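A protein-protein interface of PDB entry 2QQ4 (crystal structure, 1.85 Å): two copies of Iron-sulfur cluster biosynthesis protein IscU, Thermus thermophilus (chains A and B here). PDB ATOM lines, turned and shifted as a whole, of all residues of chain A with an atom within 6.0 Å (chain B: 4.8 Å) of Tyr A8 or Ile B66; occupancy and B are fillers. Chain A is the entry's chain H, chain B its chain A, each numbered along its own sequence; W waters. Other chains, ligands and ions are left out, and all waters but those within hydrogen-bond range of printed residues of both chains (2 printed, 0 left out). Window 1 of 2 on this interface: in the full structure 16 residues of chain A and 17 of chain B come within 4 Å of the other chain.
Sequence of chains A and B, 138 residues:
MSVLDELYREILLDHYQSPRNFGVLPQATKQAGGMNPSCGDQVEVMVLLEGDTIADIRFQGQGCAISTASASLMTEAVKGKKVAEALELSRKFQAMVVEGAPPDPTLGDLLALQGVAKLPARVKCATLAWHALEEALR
Among the printed residues, pairs that only touch across the chains: Leu A111 with Arg B122 (3.1 Å), Tyr A8 with Arg B122 (3.5 Å), Asp A109 with Cys B64 (3.6 Å), Ile A11 with Ala B65 (3.7 Å), Gln A114 with Arg B122 (3.8 Å), Tyr A8 with Ile B66 (3.9 Å) and Gly A108 with Cys B64 (3.999 Å).
The backbone NH (N) of Ala B65 sits at hydrogen-bond distance from the side-chain carboxylate (OD1) of Asp A109, at 2.9 Å.
Of the 16 printed residues of chain A, 6 touch a printed residue of chain B.
Along chain A the printed residues that touch a printed residue of chain B span positions 8 to 114.
Printed residues of chain B that touch a printed residue of chain A: Cys B64, Ala B65, Ile B66 and Arg B122.
Hydrophobic or aromatic side chains of chain B that line the printed part of chain A: Ala B65 and Ile B66.
Along chain B the printed residues that touch a printed residue of chain A span positions 64 to 122.
Among the printed residues, 8 pairs touch across the chains.
The side-chain sulfur (SG) of Cys B64 sits close to the backbone NH (N) of Ile B66, at 3.7 Å.
O of Cys B64 sits at hydrogen-bond distance from OG of Ser B67, at 2.8 Å.
The side-chain hydroxyl (OG1) of Thr B68 is in hydrogen-bond range of the backbone carbonyl oxygen (O) of Cys B64.
The backbone carbonyl oxygen of Arg B122 lies close to the side-chain sulfur of Cys B125, at 3.7 Å.
Water W2 bridges the side-chain carboxylate (OD2) of Asp A109 and the backbone NH (N) of Ala B65.
Water W1 lies within hydrogen-bond range of the side-chain carboxylate of Asp A109 (2.8 Å) and the backbone NH of Ala B65 (3.4 Å).
Of chain B, only Ile B66 and Arg B122 come within 4 Å of Tyr A8.
Of chain A, only Tyr A8 (3.9 Å) comes within 4 Å of Ile B66.
Printed residues of chain B within 4 Å of Gly A108: Cys B64 (3.999 Å).
Printed residues of chain A within 4 Å of Ala B65: Ile A11 (3.7 Å) and Asp A109 (2.9 Å).
Of the printed residues of chain B, Gln A114 touches Arg B122.
Of the printed residues of chain B, Ile A11 touches Ala B65.
The nearest printed residue of chain B that does not touch Tyr A8 is Ala B65 (6.0 Å).
No position is printed for both chains.
Of the 8 pairs that touch across the chains among the printed residues, none has its exchanged pair printed and touching as well.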
ATOM      1  N   VAL A   3      -8.294  25.803  -4.182  1.00  0.00           N
ATOM      2  CA  VAL A   3      -7.903  26.950  -4.992  1.00  0.00           C
ATOM      3  C   VAL A   3      -9.032  27.235  -5.972  1.00  0.00           C
ATOM      4  O   VAL A   3      -9.382  28.389  -6.209  1.00  0.00           O
ATOM      5  CB  VAL A   3      -6.606  26.680  -5.790  1.00  0.00           C
ATOM      6  CG1 VAL A   3      -6.338  27.830  -6.756  1.00  0.00           C
ATOM      7  CG2 VAL A   3      -5.437  26.509  -4.836  1.00  0.00           C
ATOM      8  N   LEU A   4      -9.604  26.171  -6.530  1.00  0.00           N
ATOM      9  CA  LEU A   4     -10.698  26.306  -7.480  1.00  0.00           C
ATOM     10  C   LEU A   4     -11.994  26.768  -6.813  1.00  0.00           C
ATOM     11  O   LEU A   4     -12.758  27.532  -7.399  1.00  0.00           O
ATOM     12  CB  LEU A   4     -10.928  24.986  -8.220  1.00  0.00           C
ATOM     13  CG  LEU A   4      -9.893  24.665  -9.306  1.00  0.00           C
ATOM     14  CD1 LEU A   4     -10.243  23.338  -9.965  1.00  0.00           C
ATOM     15  CD2 LEU A   4      -9.857  25.791 -10.345  1.00  0.00           C
ATOM     16  N   ASP A   5     -12.246  26.312  -5.591  1.00  0.00           N
ATOM     17  CA  ASP A   5     -13.454  26.735  -4.889  1.00  0.00           C
ATOM     18  C   ASP A   5     -13.416  28.235  -4.672  1.00  0.00           C
ATOM     19  O   ASP A   5     -14.446  28.910  -4.708  1.00  0.00           O
ATOM     20  CB  ASP A   5     -13.577  26.036  -3.536  1.00  0.00           C
ATOM     21  CG  ASP A   5     -14.120  24.635  -3.655  1.00  0.00           C
ATOM     22  OD1 ASP A   5     -14.461  24.219  -4.781  1.00  0.00           O
ATOM     23  OD2 ASP A   5     -14.208  23.950  -2.621  1.00  0.00           O
ATOM     24  N   GLU A   6     -12.216  28.758  -4.450  1.00  0.00           N
ATOM     25  CA  GLU A   6     -12.067  30.183  -4.220  1.00  0.00           C
ATOM     26  C   GLU A   6     -12.202  30.956  -5.531  1.00  0.00           C
ATOM     27  O   GLU A   6     -12.714  32.077  -5.550  1.00  0.00           O
ATOM     28  CB  GLU A   6     -10.727  30.462  -3.543  1.00  0.00           C
ATOM     29  CG  GLU A   6     -10.535  29.656  -2.267  1.00  0.00           C
ATOM     30  CD  GLU A   6      -9.621  30.332  -1.270  1.00  0.00           C
ATOM     31  OE1 GLU A   6      -8.474  30.668  -1.637  1.00  0.00           O
ATOM     32  OE2 GLU A   6     -10.051  30.523  -0.116  1.00  0.00           O
ATOM     33  N   LEU A   7     -11.743  30.358  -6.626  1.00  0.00           N
ATOM     34  CA  LEU A   7     -11.879  31.003  -7.925  1.00  0.00           C
ATOM     35  C   LEU A   7     -13.379  31.153  -8.169  1.00  0.00           C
ATOM     36  O   LEU A   7     -13.848  32.218  -8.571  1.00  0.00           O
ATOM     37  CB  LEU A   7     -11.268  30.143  -9.037  1.00  0.00           C
ATOM     38  CG  LEU A   7     -11.596  30.613 -10.460  1.00  0.00           C
ATOM     39  CD1 LEU A   7     -10.992  31.994 -10.724  1.00  0.00           C
ATOM     40  CD2 LEU A   7     -11.062  29.611 -11.447  1.00  0.00           C
ATOM     41  N   TYR A   8     -14.124  30.080  -7.912  1.00  0.00           N
ATOM     42  CA  TYR A   8     -15.580  30.082  -8.087  1.00  0.00           C
ATOM     43  C   TYR A   8     -16.238  31.162  -7.228  1.00  0.00           C
ATOM     44  O   TYR A   8     -17.131  31.870  -7.686  1.00  0.00           O
ATOM     45  CB  TYR A   8     -16.164  28.719  -7.703  1.00  0.00           C
ATOM     46  CG  TYR A   8     -15.978  27.640  -8.750  1.00  0.00           C
ATOM     47  CD1 TYR A   8     -15.881  26.298  -8.378  1.00  0.00           C
ATOM     48  CD2 TYR A   8     -15.912  27.956 -10.108  1.00  0.00           C
ATOM     49  CE1 TYR A   8     -15.720  25.293  -9.331  1.00  0.00           C
ATOM     50  CE2 TYR A   8     -15.751  26.955 -11.074  1.00  0.00           C
ATOM     51  CZ  TYR A   8     -15.656  25.626 -10.676  1.00  0.00           C
ATOM     52  OH  TYR A   8     -15.492  24.627 -11.615  1.00  0.00           O
ATOM     53  N   ARG A   9     -15.797  31.281  -5.979  1.00  0.00           N
ATOM     54  CA  ARG A   9     -16.363  32.282  -5.090  1.00  0.00           C
ATOM     55  C   ARG A   9     -16.112  33.661  -5.680  1.00  0.00           C
ATOM     56  O   ARG A   9     -16.991  34.521  -5.650  1.00  0.00           O
ATOM     57  CB  ARG A   9     -15.751  32.175  -3.689  1.00  0.00           C
ATOM     58  CG  ARG A   9     -16.424  33.076  -2.657  1.00  0.00           C
ATOM     59  CD  ARG A   9     -16.145  32.584  -1.245  1.00  0.00           C
ATOM     60  NE  ARG A   9     -14.719  32.590  -0.936  1.00  0.00           N
ATOM     61  CZ  ARG A   9     -14.122  31.690  -0.162  1.00  0.00           C
ATOM     62  NH1 ARG A   9     -12.820  31.771   0.071  1.00  0.00           N
ATOM     63  NH2 ARG A   9     -14.825  30.698   0.366  1.00  0.00           N
ATOM     64  N   GLU A  10     -14.916  33.869  -6.229  1.00  0.00           N
ATOM     65  CA  GLU A  10     -14.591  35.152  -6.846  1.00  0.00           C
ATOM     66  C   GLU A  10     -15.522  35.383  -8.023  1.00  0.00           C
ATOM     67  O   GLU A  10     -15.964  36.505  -8.265  1.00  0.00           O
ATOM     68  CB  GLU A  10     -13.138  35.176  -7.332  1.00  0.00           C
ATOM     69  CG  GLU A  10     -12.121  35.208  -6.209  1.00  0.00           C
ATOM     70  CD  GLU A  10     -12.178  36.502  -5.420  1.00  0.00           C
ATOM     71  OE1 GLU A  10     -11.591  36.553  -4.318  1.00  0.00           O
ATOM     72  OE2 GLU A  10     -12.802  37.471  -5.904  1.00  0.00           O
ATOM     73  N   ILE A  11     -15.820  34.314  -8.757  1.00  0.00           N
ATOM     74  CA  ILE A  11     -16.717  34.417  -9.904  1.00  0.00           C
ATOM     75  C   ILE A  11     -18.091  34.867  -9.419  1.00  0.00           C
ATOM     76  O   ILE A  11     -18.673  35.797  -9.970  1.00  0.00           O
ATOM     77  CB  ILE A  11     -16.843  33.064 -10.657  1.00  0.00           C
ATOM     78  CG1 ILE A  11     -15.512  32.733 -11.339  1.00  0.00           C
ATOM     79  CG2 ILE A  11     -17.959  33.144 -11.699  1.00  0.00           C
ATOM     80  CD1 ILE A  11     -15.500  31.385 -12.041  1.00  0.00           C
ATOM     81  N   LEU A  12     -18.598  34.216  -8.377  1.00  0.00           N
ATOM     82  CA  LEU A  12     -19.901  34.591  -7.826  1.00  0.00           C
ATOM     83  C   LEU A  12     -19.915  36.057  -7.412  1.00  0.00           C
ATOM     84  O   LEU A  12     -20.825  36.811  -7.770  1.00  0.00           O
ATOM     85  CB  LEU A  12     -20.248  33.729  -6.613  1.00  0.00           C
ATOM     86  CG  LEU A  12     -20.577  32.261  -6.894  1.00  0.00           C
ATOM     87  CD1 LEU A  12     -21.125  31.619  -5.638  1.00  0.00           C
ATOM     88  CD2 LEU A  12     -21.601  32.171  -8.023  1.00  0.00           C
ATOM     89  N   LEU A  13     -18.895  36.459  -6.664  1.00  0.00           N
ATOM     90  CA  LEU A  13     -18.790  37.838  -6.195  1.00  0.00           C
ATOM     91  C   LEU A  13     -18.776  38.825  -7.355  1.00  0.00           C
ATOM     92  O   LEU A  13     -19.401  39.887  -7.286  1.00  0.00           O
ATOM     93  CB  LEU A  13     -17.524  38.010  -5.345  1.00  0.00           C
ATOM     94  CG  LEU A  13     -17.484  37.225  -4.029  1.00  0.00           C
ATOM     95  CD1 LEU A  13     -16.134  37.405  -3.344  1.00  0.00           C
ATOM     96  CD2 LEU A  13     -18.604  37.713  -3.122  1.00  0.00           C
ATOM     97  N   GLY A 108     -20.113  24.680 -16.778  1.00  0.00           N
ATOM     98  CA  GLY A 108     -19.069  25.686 -16.722  1.00  0.00           C
ATOM     99  C   GLY A 108     -19.036  26.530 -15.467  1.00  0.00           C
ATOM    100  O   GLY A 108     -18.987  26.007 -14.356  1.00  0.00           O
ATOM    101  N   ASP A 109     -19.056  27.844 -15.646  1.00  0.00           N
ATOM    102  CA  ASP A 109     -19.013  28.757 -14.520  1.00  0.00           C
ATOM    103  C   ASP A 109     -20.193  28.573 -13.575  1.00  0.00           C
ATOM    104  O   ASP A 109     -20.116  28.951 -12.412  1.00  0.00           O
ATOM    105  CB  ASP A 109     -18.944  30.202 -15.013  1.00  0.00           C
ATOM    106  CG  ASP A 109     -17.614  30.525 -15.677  1.00  0.00           C
ATOM    107  OD1 ASP A 109     -16.677  29.702 -15.559  1.00  0.00           O
ATOM    108  OD2 ASP A 109     -17.503  31.598 -16.306  1.00  0.00           O
ATOM    109  N   LEU A 111     -21.031  26.045 -12.242  1.00  0.00           N
ATOM    110  CA  LEU A 111     -20.615  25.127 -11.192  1.00  0.00           C
ATOM    111  C   LEU A 111     -20.317  25.881  -9.893  1.00  0.00           C
ATOM    112  O   LEU A 111     -20.297  25.293  -8.815  1.00  0.00           O
ATOM    113  CB  LEU A 111     -19.387  24.330 -11.641  1.00  0.00           C
ATOM    114  CG  LEU A 111     -19.657  23.331 -12.773  1.00  0.00           C
ATOM    115  CD1 LEU A 111     -18.380  22.574 -13.121  1.00  0.00           C
ATOM    116  CD2 LEU A 111     -20.744  22.358 -12.338  1.00  0.00           C
ATOM    117  N   ALA A 112     -20.099  27.186  -9.999  1.00  0.00           N
ATOM    118  CA  ALA A 112     -19.811  28.000  -8.825  1.00  0.00           C
ATOM    119  C   ALA A 112     -20.915  27.875  -7.776  1.00  0.00           C
ATOM    120  O   ALA A 112     -20.655  27.982  -6.579  1.00  0.00           O
ATOM    121  CB  ALA A 112     -19.640  29.458  -9.229  1.00  0.00           C
ATOM    122  N   GLN A 114     -22.665  25.166  -7.168  1.00  0.00           N
ATOM    123  CA  GLN A 114     -22.885  23.761  -6.841  1.00  0.00           C
ATOM    124  C   GLN A 114     -23.178  23.502  -5.363  1.00  0.00           C
ATOM    125  O   GLN A 114     -23.935  22.592  -5.026  1.00  0.00           O
ATOM    126  CB  GLN A 114     -21.680  22.920  -7.263  1.00  0.00           C
ATOM    127  CG  GLN A 114     -21.684  21.524  -6.670  1.00  0.00           C
ATOM    128  CD  GLN A 114     -20.567  20.653  -7.202  1.00  0.00           C
ATOM    129  OE1 GLN A 114     -19.431  21.105  -7.371  1.00  0.00           O
ATOM    130  NE2 GLN A 114     -20.882  19.387  -7.459  1.00  0.00           N
ATOM    131  N   CYS B  64     -15.494  28.387 -20.249  1.00  0.00           N
ATOM    132  CA  CYS B  64     -15.499  28.548 -18.805  1.00  0.00           C
ATOM    133  C   CYS B  64     -14.211  29.209 -18.323  1.00  0.00           C
ATOM    134  O   CYS B  64     -13.200  29.236 -19.034  1.00  0.00           O
ATOM    135  CB  CYS B  64     -15.647  27.188 -18.144  1.00  0.00           C
ATOM    136  SG  CYS B  64     -14.175  26.158 -18.314  1.00  0.00           S
ATOM    137  N   ALA B  65     -14.264  29.740 -17.108  1.00  0.00           N
ATOM    138  CA  ALA B  65     -13.122  30.410 -16.500  1.00  0.00           C
ATOM    139  C   ALA B  65     -11.860  29.543 -16.504  1.00  0.00           C
ATOM    140  O   ALA B  65     -10.766  30.035 -16.753  1.00  0.00           O
ATOM    141  CB  ALA B  65     -13.473  30.808 -15.057  1.00  0.00           C
ATOM    142  N   ILE B  66     -12.003  28.262 -16.193  1.00  0.00           N
ATOM    143  CA  ILE B  66     -10.844  27.374 -16.171  1.00  0.00           C
ATOM    144  C   ILE B  66     -10.167  27.293 -17.539  1.00  0.00           C
ATOM    145  O   ILE B  66      -8.946  27.380 -17.629  1.00  0.00           O
ATOM    146  CB  ILE B  66     -11.221  25.937 -15.731  1.00  0.00           C
ATOM    147  CG1 ILE B  66     -11.700  25.939 -14.274  1.00  0.00           C
ATOM    148  CG2 ILE B  66     -10.017  25.012 -15.906  1.00  0.00           C
ATOM    149  CD1 ILE B  66     -12.330  24.623 -13.832  1.00  0.00           C
ATOM    150  N   SER B  67     -10.949  27.133 -18.605  1.00  0.00           N
ATOM    151  CA  SER B  67     -10.339  27.026 -19.935  1.00  0.00           C
ATOM    152  C   SER B  67      -9.630  28.306 -20.353  1.00  0.00           C
ATOM    153  O   SER B  67      -8.570  28.258 -20.957  1.00  0.00           O
ATOM    154  CB  SER B  67     -11.377  26.623 -20.998  1.00  0.00           C
ATOM    155  OG  SER B  67     -12.452  27.543 -21.087  1.00  0.00           O
ATOM    156  N   THR B  68     -10.205  29.456 -20.015  1.00  0.00           N
ATOM    157  CA  THR B  68      -9.593  30.730 -20.379  1.00  0.00           C
ATOM    158  C   THR B  68      -8.271  30.921 -19.641  1.00  0.00           C
ATOM    159  O   THR B  68      -7.240  31.230 -20.253  1.00  0.00           O
ATOM    160  CB  THR B  68     -10.544  31.902 -20.059  1.00  0.00           C
ATOM    161  OG1 THR B  68     -11.767  31.732 -20.789  1.00  0.00           O
ATOM    162  CG2 THR B  68      -9.911  33.224 -20.456  1.00  0.00           C
ATOM    163  N   ALA B  69      -8.299  30.729 -18.325  1.00  0.00           N
ATOM    164  CA  ALA B  69      -7.094  30.879 -17.522  1.00  0.00           C
ATOM    165  C   ALA B  69      -6.031  29.912 -18.021  1.00  0.00           C
ATOM    166  O   ALA B  69      -4.864  30.263 -18.186  1.00  0.00           O
ATOM    167  CB  ALA B  69      -7.397  30.592 -16.077  1.00  0.00           C
ATOM    168  N   SER B  70      -6.431  28.672 -18.266  1.00  0.00           N
ATOM    169  CA  SER B  70      -5.443  27.718 -18.718  1.00  0.00           C
ATOM    170  C   SER B  70      -4.804  28.140 -20.038  1.00  0.00           C
ATOM    171  O   SER B  70      -3.586  28.080 -20.180  1.00  0.00           O
ATOM    172  CB  SER B  70      -6.051  26.319 -18.846  1.00  0.00           C
ATOM    173  OG  SER B  70      -5.015  25.379 -19.063  1.00  0.00           O
ATOM    174  N   LEU B 113      -3.045  25.357 -11.493  1.00  0.00           N
ATOM    175  CA  LEU B 113      -4.143  24.494 -11.931  1.00  0.00           C
ATOM    176  C   LEU B 113      -4.032  23.056 -11.412  1.00  0.00           C
ATOM    177  O   LEU B 113      -4.862  22.207 -11.740  1.00  0.00           O
ATOM    178  CB  LEU B 113      -4.243  24.507 -13.465  1.00  0.00           C
ATOM    179  CG  LEU B 113      -4.754  25.838 -14.050  1.00  0.00           C
ATOM    180  CD1 LEU B 113      -4.464  25.924 -15.536  1.00  0.00           C
ATOM    181  CD2 LEU B 113      -6.262  25.960 -13.772  1.00  0.00           C
ATOM    182  N   ARG B 122     -13.622  18.003 -15.067  1.00  0.00           N
ATOM    183  CA  ARG B 122     -13.229  19.343 -15.513  1.00  0.00           C
ATOM    184  C   ARG B 122     -11.795  19.389 -16.071  1.00  0.00           C
ATOM    185  O   ARG B 122     -11.324  20.427 -16.551  1.00  0.00           O
ATOM    186  CB  ARG B 122     -13.359  20.336 -14.349  1.00  0.00           C
ATOM    187  CG  ARG B 122     -14.768  20.434 -13.764  1.00  0.00           C
ATOM    188  CD  ARG B 122     -14.731  21.154 -12.420  1.00  0.00           C
ATOM    189  NE  ARG B 122     -16.004  21.129 -11.695  1.00  0.00           N
ATOM    190  CZ  ARG B 122     -16.621  20.026 -11.276  1.00  0.00           C
ATOM    191  NH1 ARG B 122     -16.095  18.829 -11.509  1.00  0.00           N
ATOM    192  NH2 ARG B 122     -17.764  20.119 -10.609  1.00  0.00           N
ATOM    193  N   CYS B 125     -11.271  20.910 -19.425  1.00  0.00           N
ATOM    194  CA  CYS B 125     -11.314  22.358 -19.548  1.00  0.00           C
ATOM    195  C   CYS B 125      -9.899  22.920 -19.445  1.00  0.00           C
ATOM    196  O   CYS B 125      -9.576  23.940 -20.069  1.00  0.00           O
ATOM    197  CB  CYS B 125     -12.206  22.949 -18.451  1.00  0.00           C
ATOM    198  SG  CYS B 125     -13.892  22.328 -18.494  1.00  0.00           S
ATOM    199  N   ALA B 126      -9.050  22.246 -18.671  1.00  0.00           N
ATOM    200  CA  ALA B 126      -7.667  22.695 -18.486  1.00  0.00           C
ATOM    201  C   ALA B 126      -6.730  22.272 -19.621  1.00  0.00           C
ATOM    202  O   ALA B 126      -5.828  23.014 -19.992  1.00  0.00           O
ATOM    203  CB  ALA B 126      -7.121  22.177 -17.152  1.00  0.00           C
HETATM  204  O   HOH W   1     -15.175  27.514 -14.705  1.00  0.00           O
HETATM  205  O   HOH W   2     -16.016  32.411 -18.193  1.00  0.00           O
